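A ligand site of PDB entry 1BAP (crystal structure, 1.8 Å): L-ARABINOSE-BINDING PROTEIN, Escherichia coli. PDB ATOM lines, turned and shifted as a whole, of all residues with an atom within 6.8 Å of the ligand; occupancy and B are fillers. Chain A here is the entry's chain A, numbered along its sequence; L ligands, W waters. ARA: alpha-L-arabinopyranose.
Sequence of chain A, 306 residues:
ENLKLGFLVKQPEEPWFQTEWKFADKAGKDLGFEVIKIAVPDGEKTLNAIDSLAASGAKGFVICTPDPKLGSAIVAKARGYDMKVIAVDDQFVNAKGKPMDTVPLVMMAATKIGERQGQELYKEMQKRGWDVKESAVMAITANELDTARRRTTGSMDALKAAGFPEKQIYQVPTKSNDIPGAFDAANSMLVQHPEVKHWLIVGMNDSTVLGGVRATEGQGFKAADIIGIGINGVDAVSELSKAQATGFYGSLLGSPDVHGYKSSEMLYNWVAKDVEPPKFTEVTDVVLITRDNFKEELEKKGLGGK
O4 of the ligand is in hydrogen-bond range of OD1 of Asn 232 (2.7 Å). The side-chain carboxylate (OD2) of Asp 90 lies within hydrogen-bond range of an oxygen (O1) of the ligand (2.7 Å). NH2 of Arg 151 sits at hydrogen-bond distance from O4 of the ligand (2.7 Å). OE2 of Glu 14 is in hydrogen-bond range of O3 of the ligand (2.9 Å). O2 of the ligand sits at hydrogen-bond distance from NZ of Lys 10. An oxygen (O3) of the ligand is in hydrogen-bond range of the side-chain amide nitrogen (ND2) of Asn 205.
The side-chain hydroxyl (OG1) of Thr 147 sits at hydrogen-bond distance from the guanidinium group (NH1) of Arg 151. The backbone carbonyl oxygen (O) of Met 204 is in hydrogen-bond range of the guanidinium group (NH2) of Arg 151 (2.8 Å). ND2 of Asn 205 is in hydrogen-bond range of OE1 of Glu 14. The side-chain amide oxygen of Asn 205 lies close to the backbone NH of Ser 207. The indole nitrogen (NE1) of Trp 16 lies within hydrogen-bond range of the side-chain carboxylate (OD1) of Asp 89. The backbone NH of Trp 16 sits at hydrogen-bond distance from the side-chain carboxylate of Asp 235 (2.7 Å). The side-chain carboxylate of Asp 89 lies close to the side-chain carboxylate of Glu 20, at 2.6 Å. A ring nitrogen (ND1) of His 259 is in hydrogen-bond range of the side-chain carboxylate of Asp 89.
Trp 16 touches the ligand (NE1 to C5, 3.5 Å). Asp 89 touches the ligand (CB to O5, 3.9 Å). Met 108 touches the ligand (CE to O4, 3.9 Å). CD2 of Leu 145 touches O1 of the ligand, 3.99 Å away. Thr 147 touches the ligand (CG2 to O1, 3.3 Å). CE of Met 204 touches O2 of the ligand (3.7 Å). Hydrophobic or aromatic side chains within 4 Å of the ligand: Trp 16, Met 108, Leu 145 and Met 204.
Water W2 lies within hydrogen-bond range of O2 of the ligand (2.5 Å), OE1 of Glu 14 (2.6 Å), OE1 of Gln 11 (3.0 Å) and ND2 of Asn 205 (3.0 Å). Water W1 lies within hydrogen-bond range of the side-chain hydroxyl (OG1) of Thr 147, the backbone carbonyl oxygen (O) of Asp 89, an oxygen (O5) of the ligand and the guanidinium group (NH1) of Arg 151.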
ATOM      1  N   LYS A  10      13.700 -19.983  15.309  1.00  0.00           N
ATOM      2  CA  LYS A  10      12.573 -20.910  15.092  1.00  0.00           C
ATOM      3  C   LYS A  10      12.567 -21.507  13.695  1.00  0.00           C
ATOM      4  O   LYS A  10      12.112 -22.658  13.549  1.00  0.00           O
ATOM      5  CB  LYS A  10      11.225 -20.245  15.393  1.00  0.00           C
ATOM      6  CG  LYS A  10      10.959 -19.001  14.563  1.00  0.00           C
ATOM      7  CD  LYS A  10       9.597 -18.379  14.905  1.00  0.00           C
ATOM      8  CE  LYS A  10       9.209 -17.310  13.911  1.00  0.00           C
ATOM      9  NZ  LYS A  10       7.832 -16.826  14.163  1.00  0.00           N
ATOM     10  N   GLN A  11      12.950 -20.730  12.699  1.00  0.00           N
ATOM     11  CA  GLN A  11      12.862 -21.142  11.288  1.00  0.00           C
ATOM     12  C   GLN A  11      14.151 -20.834  10.534  1.00  0.00           C
ATOM     13  O   GLN A  11      14.265 -19.802   9.859  1.00  0.00           O
ATOM     14  CB  GLN A  11      11.613 -20.556  10.610  1.00  0.00           C
ATOM     15  CG  GLN A  11      10.316 -21.052  11.240  1.00  0.00           C
ATOM     16  CD  GLN A  11       9.060 -20.440  10.647  1.00  0.00           C
ATOM     17  OE1 GLN A  11       8.244 -19.840  11.351  1.00  0.00           O
ATOM     18  NE2 GLN A  11       8.731 -20.906   9.439  1.00  0.00           N
ATOM     19  N   GLU A  14      14.284 -19.875   6.635  1.00  0.00           N
ATOM     20  CA  GLU A  14      13.923 -18.529   6.151  1.00  0.00           C
ATOM     21  C   GLU A  14      15.208 -17.698   6.004  1.00  0.00           C
ATOM     22  O   GLU A  14      15.924 -17.520   7.009  1.00  0.00           O
ATOM     23  CB  GLU A  14      13.039 -17.788   7.149  1.00  0.00           C
ATOM     24  CG  GLU A  14      11.542 -18.048   7.131  1.00  0.00           C
ATOM     25  CD  GLU A  14      10.634 -17.067   7.799  1.00  0.00           C
ATOM     26  OE1 GLU A  14       9.414 -17.195   7.824  1.00  0.00           O
ATOM     27  OE2 GLU A  14      11.214 -16.018   8.183  1.00  0.00           O
ATOM     28  N   TRP A  16      15.295 -14.585   6.225  1.00  0.00           N
ATOM     29  CA  TRP A  16      15.199 -13.649   7.363  1.00  0.00           C
ATOM     30  C   TRP A  16      16.151 -14.053   8.488  1.00  0.00           C
ATOM     31  O   TRP A  16      16.943 -13.233   8.984  1.00  0.00           O
ATOM     32  CB  TRP A  16      13.763 -13.516   7.857  1.00  0.00           C
ATOM     33  CG  TRP A  16      13.586 -12.626   9.038  1.00  0.00           C
ATOM     34  CD1 TRP A  16      13.553 -12.999  10.357  1.00  0.00           C
ATOM     35  CD2 TRP A  16      13.377 -11.211   9.018  1.00  0.00           C
ATOM     36  NE1 TRP A  16      13.414 -11.890  11.162  1.00  0.00           N
ATOM     37  CE2 TRP A  16      13.318 -10.776  10.363  1.00  0.00           C
ATOM     38  CE3 TRP A  16      13.285 -10.276   7.989  1.00  0.00           C
ATOM     39  CZ2 TRP A  16      13.148  -9.446  10.703  1.00  0.00           C
ATOM     40  CZ3 TRP A  16      13.124  -8.948   8.332  1.00  0.00           C
ATOM     41  CH2 TRP A  16      13.075  -8.530   9.665  1.00  0.00           C
ATOM     42  N   PHE A  17      16.003 -15.297   8.922  1.00  0.00           N
ATOM     43  CA  PHE A  17      16.735 -15.854  10.081  1.00  0.00           C
ATOM     44  C   PHE A  17      18.184 -16.154   9.735  1.00  0.00           C
ATOM     45  O   PHE A  17      19.087 -15.967  10.567  1.00  0.00           O
ATOM     46  CB  PHE A  17      16.004 -17.040  10.703  1.00  0.00           C
ATOM     47  CG  PHE A  17      14.801 -16.669  11.525  1.00  0.00           C
ATOM     48  CD1 PHE A  17      13.520 -17.001  11.080  1.00  0.00           C
ATOM     49  CD2 PHE A  17      14.919 -15.759  12.580  1.00  0.00           C
ATOM     50  CE1 PHE A  17      12.393 -16.569  11.747  1.00  0.00           C
ATOM     51  CE2 PHE A  17      13.795 -15.299  13.262  1.00  0.00           C
ATOM     52  CZ  PHE A  17      12.524 -15.716  12.843  1.00  0.00           C
ATOM     53  N   GLU A  20      19.964 -12.904  10.108  1.00  0.00           N
ATOM     54  CA  GLU A  20      20.201 -12.608  11.522  1.00  0.00           C
ATOM     55  C   GLU A  20      21.416 -13.352  12.046  1.00  0.00           C
ATOM     56  O   GLU A  20      22.337 -12.727  12.607  1.00  0.00           O
ATOM     57  CB  GLU A  20      18.985 -12.958  12.386  1.00  0.00           C
ATOM     58  CG  GLU A  20      17.768 -12.056  12.168  1.00  0.00           C
ATOM     59  CD  GLU A  20      16.658 -12.165  13.176  1.00  0.00           C
ATOM     60  OE1 GLU A  20      15.730 -11.384  13.245  1.00  0.00           O
ATOM     61  OE2 GLU A  20      16.777 -13.170  13.898  1.00  0.00           O
ATOM     62  N   CYS A  64      14.753 -16.348  18.999  1.00  0.00           N
ATOM     63  CA  CYS A  64      13.402 -16.247  18.426  1.00  0.00           C
ATOM     64  C   CYS A  64      12.683 -17.588  18.642  1.00  0.00           C
ATOM     65  O   CYS A  64      12.911 -18.572  17.913  1.00  0.00           O
ATOM     66  CB  CYS A  64      13.370 -15.839  16.962  1.00  0.00           C
ATOM     67  SG  CYS A  64      11.678 -15.560  16.366  1.00  0.00           S
ATOM     68  N   VAL A  88      14.520 -11.932  20.209  1.00  0.00           N
ATOM     69  CA  VAL A  88      14.476 -11.258  18.905  1.00  0.00           C
ATOM     70  C   VAL A  88      13.212 -11.687  18.164  1.00  0.00           C
ATOM     71  O   VAL A  88      12.771 -12.849  18.251  1.00  0.00           O
ATOM     72  CB  VAL A  88      15.777 -11.496  18.108  1.00  0.00           C
ATOM     73  CG1 VAL A  88      15.860 -12.881  17.500  1.00  0.00           C
ATOM     74  CG2 VAL A  88      15.987 -10.423  17.047  1.00  0.00           C
ATOM     75  N   ASP A  89      12.531 -10.683  17.644  1.00  0.00           N
ATOM     76  CA  ASP A  89      11.339 -10.832  16.800  1.00  0.00           C
ATOM     77  C   ASP A  89      10.063 -11.094  17.594  1.00  0.00           C
ATOM     78  O   ASP A  89       9.048 -10.423  17.337  1.00  0.00           O
ATOM     79  CB  ASP A  89      11.578 -11.785  15.639  1.00  0.00           C
ATOM     80  CG  ASP A  89      12.732 -11.386  14.740  1.00  0.00           C
ATOM     81  OD1 ASP A  89      13.572 -12.221  14.403  1.00  0.00           O
ATOM     82  OD2 ASP A  89      12.800 -10.172  14.430  1.00  0.00           O
ATOM     83  N   ASP A  90      10.025 -12.261  18.207  1.00  0.00           N
ATOM     84  CA  ASP A  90       8.825 -12.788  18.881  1.00  0.00           C
ATOM     85  C   ASP A  90       8.951 -12.621  20.390  1.00  0.00           C
ATOM     86  O   ASP A  90       9.748 -13.342  21.026  1.00  0.00           O
ATOM     87  CB  ASP A  90       8.568 -14.236  18.468  1.00  0.00           C
ATOM     88  CG  ASP A  90       8.284 -14.433  16.987  1.00  0.00           C
ATOM     89  OD1 ASP A  90       7.970 -15.554  16.550  1.00  0.00           O
ATOM     90  OD2 ASP A  90       8.532 -13.470  16.227  1.00  0.00           O
ATOM     91  N   MET A 108      10.774  -5.578  14.877  1.00  0.00           N
ATOM     92  CA  MET A 108      10.285  -4.636  13.877  1.00  0.00           C
ATOM     93  C   MET A 108       9.098  -3.865  14.467  1.00  0.00           C
ATOM     94  O   MET A 108       8.492  -4.320  15.441  1.00  0.00           O
ATOM     95  CB  MET A 108       9.941  -5.327  12.566  1.00  0.00           C
ATOM     96  CG  MET A 108       8.731  -6.222  12.693  1.00  0.00           C
ATOM     97  SD  MET A 108       8.160  -6.671  11.007  1.00  0.00           S
ATOM     98  CE  MET A 108       9.492  -7.775  10.504  1.00  0.00           C
ATOM     99  N   LEU A 145      -0.025 -15.329  17.570  1.00  0.00           N
ATOM    100  CA  LEU A 145       1.292 -14.674  17.606  1.00  0.00           C
ATOM    101  C   LEU A 145       1.128 -13.161  17.464  1.00  0.00           C
ATOM    102  O   LEU A 145       0.773 -12.641  16.388  1.00  0.00           O
ATOM    103  CB  LEU A 145       2.163 -15.302  16.513  1.00  0.00           C
ATOM    104  CG  LEU A 145       3.573 -14.742  16.365  1.00  0.00           C
ATOM    105  CD1 LEU A 145       4.381 -14.960  17.643  1.00  0.00           C
ATOM    106  CD2 LEU A 145       4.262 -15.393  15.168  1.00  0.00           C
ATOM    107  N   THR A 147       3.057 -10.543  17.143  1.00  0.00           N
ATOM    108  CA  THR A 147       3.782  -9.822  16.080  1.00  0.00           C
ATOM    109  C   THR A 147       3.056  -9.969  14.740  1.00  0.00           C
ATOM    110  O   THR A 147       2.989  -8.990  13.960  1.00  0.00           O
ATOM    111  CB  THR A 147       5.291 -10.257  15.977  1.00  0.00           C
ATOM    112  OG1 THR A 147       5.929  -9.300  15.074  1.00  0.00           O
ATOM    113  CG2 THR A 147       5.498 -11.700  15.510  1.00  0.00           C
ATOM    114  N   ALA A 148       2.564 -11.162  14.496  1.00  0.00           N
ATOM    115  CA  ALA A 148       1.830 -11.506  13.275  1.00  0.00           C
ATOM    116  C   ALA A 148       0.469 -10.790  13.276  1.00  0.00           C
ATOM    117  O   ALA A 148       0.136 -10.099  12.299  1.00  0.00           O
ATOM    118  CB  ALA A 148       1.661 -13.003  13.134  1.00  0.00           C
ATOM    119  N   ARG A 151       0.682  -6.980  12.590  1.00  0.00           N
ATOM    120  CA  ARG A 151       0.925  -6.748  11.159  1.00  0.00           C
ATOM    121  C   ARG A 151      -0.369  -6.804  10.349  1.00  0.00           C
ATOM    122  O   ARG A 151      -0.644  -5.883   9.553  1.00  0.00           O
ATOM    123  CB  ARG A 151       1.972  -7.692  10.568  1.00  0.00           C
ATOM    124  CG  ARG A 151       3.416  -7.188  10.682  1.00  0.00           C
ATOM    125  CD  ARG A 151       4.390  -8.232  10.272  1.00  0.00           C
ATOM    126  NE  ARG A 151       4.758  -9.076  11.410  1.00  0.00           N
ATOM    127  CZ  ARG A 151       5.798  -9.927  11.369  1.00  0.00           C
ATOM    128  NH1 ARG A 151       6.216 -10.539  12.465  1.00  0.00           N
ATOM    129  NH2 ARG A 151       6.362 -10.213  10.192  1.00  0.00           N
ATOM    130  N   ASN A 177       3.009 -21.005   9.811  1.00  0.00           N
ATOM    131  CA  ASN A 177       3.491 -19.743   9.225  1.00  0.00           C
ATOM    132  C   ASN A 177       4.465 -20.044   8.082  1.00  0.00           C
ATOM    133  O   ASN A 177       5.627 -19.596   8.136  1.00  0.00           O
ATOM    134  CB  ASN A 177       4.079 -18.819  10.285  1.00  0.00           C
ATOM    135  CG  ASN A 177       3.089 -18.428  11.355  1.00  0.00           C
ATOM    136  OD1 ASN A 177       1.882 -18.305  11.083  1.00  0.00           O
ATOM    137  ND2 ASN A 177       3.569 -18.277  12.578  1.00  0.00           N
ATOM    138  N   MET A 204       1.318 -11.836   7.318  1.00  0.00           N
ATOM    139  CA  MET A 204       2.321 -11.208   8.184  1.00  0.00           C
ATOM    140  C   MET A 204       3.722 -11.243   7.582  1.00  0.00           C
ATOM    141  O   MET A 204       4.575 -10.436   8.008  1.00  0.00           O
ATOM    142  CB  MET A 204       2.259 -11.763   9.595  1.00  0.00           C
ATOM    143  CG  MET A 204       2.687 -13.205   9.658  1.00  0.00           C
ATOM    144  SD  MET A 204       4.307 -13.288  10.509  1.00  0.00           S
ATOM    145  CE  MET A 204       4.412 -15.070  10.757  1.00  0.00           C
ATOM    146  N   ASN A 205       3.976 -12.157   6.660  1.00  0.00           N
ATOM    147  CA  ASN A 205       5.339 -12.316   6.094  1.00  0.00           C
ATOM    148  C   ASN A 205       5.288 -12.847   4.659  1.00  0.00           C
ATOM    149  O   ASN A 205       4.221 -13.197   4.137  1.00  0.00           O
ATOM    150  CB  ASN A 205       6.227 -13.103   7.046  1.00  0.00           C
ATOM    151  CG  ASN A 205       5.888 -14.576   7.170  1.00  0.00           C
ATOM    152  OD1 ASN A 205       5.063 -15.113   6.414  1.00  0.00           O
ATOM    153  ND2 ASN A 205       6.607 -15.267   8.055  1.00  0.00           N
ATOM    154  N   ASP A 206       6.459 -12.860   4.048  1.00  0.00           N
ATOM    155  CA  ASP A 206       6.648 -13.323   2.676  1.00  0.00           C
ATOM    156  C   ASP A 206       6.000 -14.694   2.448  1.00  0.00           C
ATOM    157  O   ASP A 206       5.359 -14.883   1.399  1.00  0.00           O
ATOM    158  CB  ASP A 206       8.127 -13.260   2.272  1.00  0.00           C
ATOM    159  CG  ASP A 206       8.627 -11.841   2.034  1.00  0.00           C
ATOM    160  OD1 ASP A 206       7.869 -10.953   1.612  1.00  0.00           O
ATOM    161  OD2 ASP A 206       9.815 -11.608   2.365  1.00  0.00           O
ATOM    162  N   SER A 207       6.376 -15.653   3.267  1.00  0.00           N
ATOM    163  CA  SER A 207       5.955 -17.053   3.086  1.00  0.00           C
ATOM    164  C   SER A 207       4.433 -17.174   3.073  1.00  0.00           C
ATOM    165  O   SER A 207       3.866 -17.960   2.295  1.00  0.00           O
ATOM    166  CB  SER A 207       6.566 -17.975   4.136  1.00  0.00           C
ATOM    167  OG  SER A 207       7.901 -18.329   3.757  1.00  0.00           O
ATOM    168  N   ILE A 231       6.120  -9.247   3.696  1.00  0.00           N
ATOM    169  CA  ILE A 231       6.985  -8.542   4.667  1.00  0.00           C
ATOM    170  C   ILE A 231       8.204  -9.434   4.960  1.00  0.00           C
ATOM    171  O   ILE A 231       8.043 -10.640   5.190  1.00  0.00           O
ATOM    172  CB  ILE A 231       6.194  -8.199   5.966  1.00  0.00           C
ATOM    173  CG1 ILE A 231       5.015  -7.236   5.647  1.00  0.00           C
ATOM    174  CG2 ILE A 231       7.105  -7.620   7.086  1.00  0.00           C
ATOM    175  CD1 ILE A 231       4.094  -6.946   6.857  1.00  0.00           C
ATOM    176  N   ASN A 232       9.367  -8.817   4.892  1.00  0.00           N
ATOM    177  CA  ASN A 232      10.667  -9.403   5.224  1.00  0.00           C
ATOM    178  C   ASN A 232      11.700  -8.932   4.184  1.00  0.00           C
ATOM    179  O   ASN A 232      12.806  -8.493   4.524  1.00  0.00           O
ATOM    180  CB  ASN A 232      10.668 -10.904   5.450  1.00  0.00           C
ATOM    181  CG  ASN A 232      10.191 -11.318   6.830  1.00  0.00           C
ATOM    182  OD1 ASN A 232       9.743 -10.482   7.630  1.00  0.00           O
ATOM    183  ND2 ASN A 232      10.061 -12.626   7.035  1.00  0.00           N
ATOM    184  N   ASP A 235      13.182 -12.750   2.105  1.00  0.00           N
ATOM    185  CA  ASP A 235      12.510 -14.032   1.862  1.00  0.00           C
ATOM    186  C   ASP A 235      11.934 -14.098   0.431  1.00  0.00           C
ATOM    187  O   ASP A 235      11.445 -15.173   0.045  1.00  0.00           O
ATOM    188  CB  ASP A 235      11.452 -14.357   2.913  1.00  0.00           C
ATOM    189  CG  ASP A 235      11.979 -14.591   4.313  1.00  0.00           C
ATOM    190  OD1 ASP A 235      13.186 -14.521   4.566  1.00  0.00           O
ATOM    191  OD2 ASP A 235      11.121 -14.822   5.193  1.00  0.00           O
ATOM    192  N   HIS A 259      18.750  -6.556  13.389  1.00  0.00           N
ATOM    193  CA  HIS A 259      18.249  -7.458  14.434  1.00  0.00           C
ATOM    194  C   HIS A 259      19.339  -8.420  14.904  1.00  0.00           C
ATOM    195  O   HIS A 259      19.559  -8.557  16.123  1.00  0.00           O
ATOM    196  CB  HIS A 259      16.984  -8.254  14.048  1.00  0.00           C
ATOM    197  CG  HIS A 259      15.764  -7.421  13.771  1.00  0.00           C
ATOM    198  ND1 HIS A 259      14.489  -7.923  13.781  1.00  0.00           N
ATOM    199  CD2 HIS A 259      15.654  -6.136  13.363  1.00  0.00           C
ATOM    200  CE1 HIS A 259      13.654  -6.985  13.379  1.00  0.00           C
ATOM    201  NE2 HIS A 259      14.334  -5.888  13.121  1.00  0.00           N
HETATM  202  C1  ARA L   1       8.674 -13.447  12.913  1.00  0.00           C
HETATM  203  C2  ARA L   1       8.322 -14.014  11.537  1.00  0.00           C
HETATM  204  C3  ARA L   1       9.475 -13.752  10.575  1.00  0.00           C
HETATM  205  C4  ARA L   1       9.775 -12.249  10.505  1.00  0.00           C
HETATM  206  C5  ARA L   1      10.037 -11.732  11.913  1.00  0.00           C
HETATM  207  O1  ARA L   1       7.528 -13.594  13.749  1.00  0.00           O
HETATM  208  O2  ARA L   1       7.999 -15.400  11.621  1.00  0.00           O
HETATM  209  O3  ARA L   1       9.203 -14.249   9.259  1.00  0.00           O
HETATM  210  O4  ARA L   1       8.735 -11.511   9.863  1.00  0.00           O
HETATM  211  O5  ARA L   1       8.936 -12.042  12.796  1.00  0.00           O
HETATM  212  O   HOH W   1       8.416  -9.936  14.704  1.00  0.00           O
HETATM  213  O   HOH W   2       7.943 -17.224   9.919  1.00  0.00           O
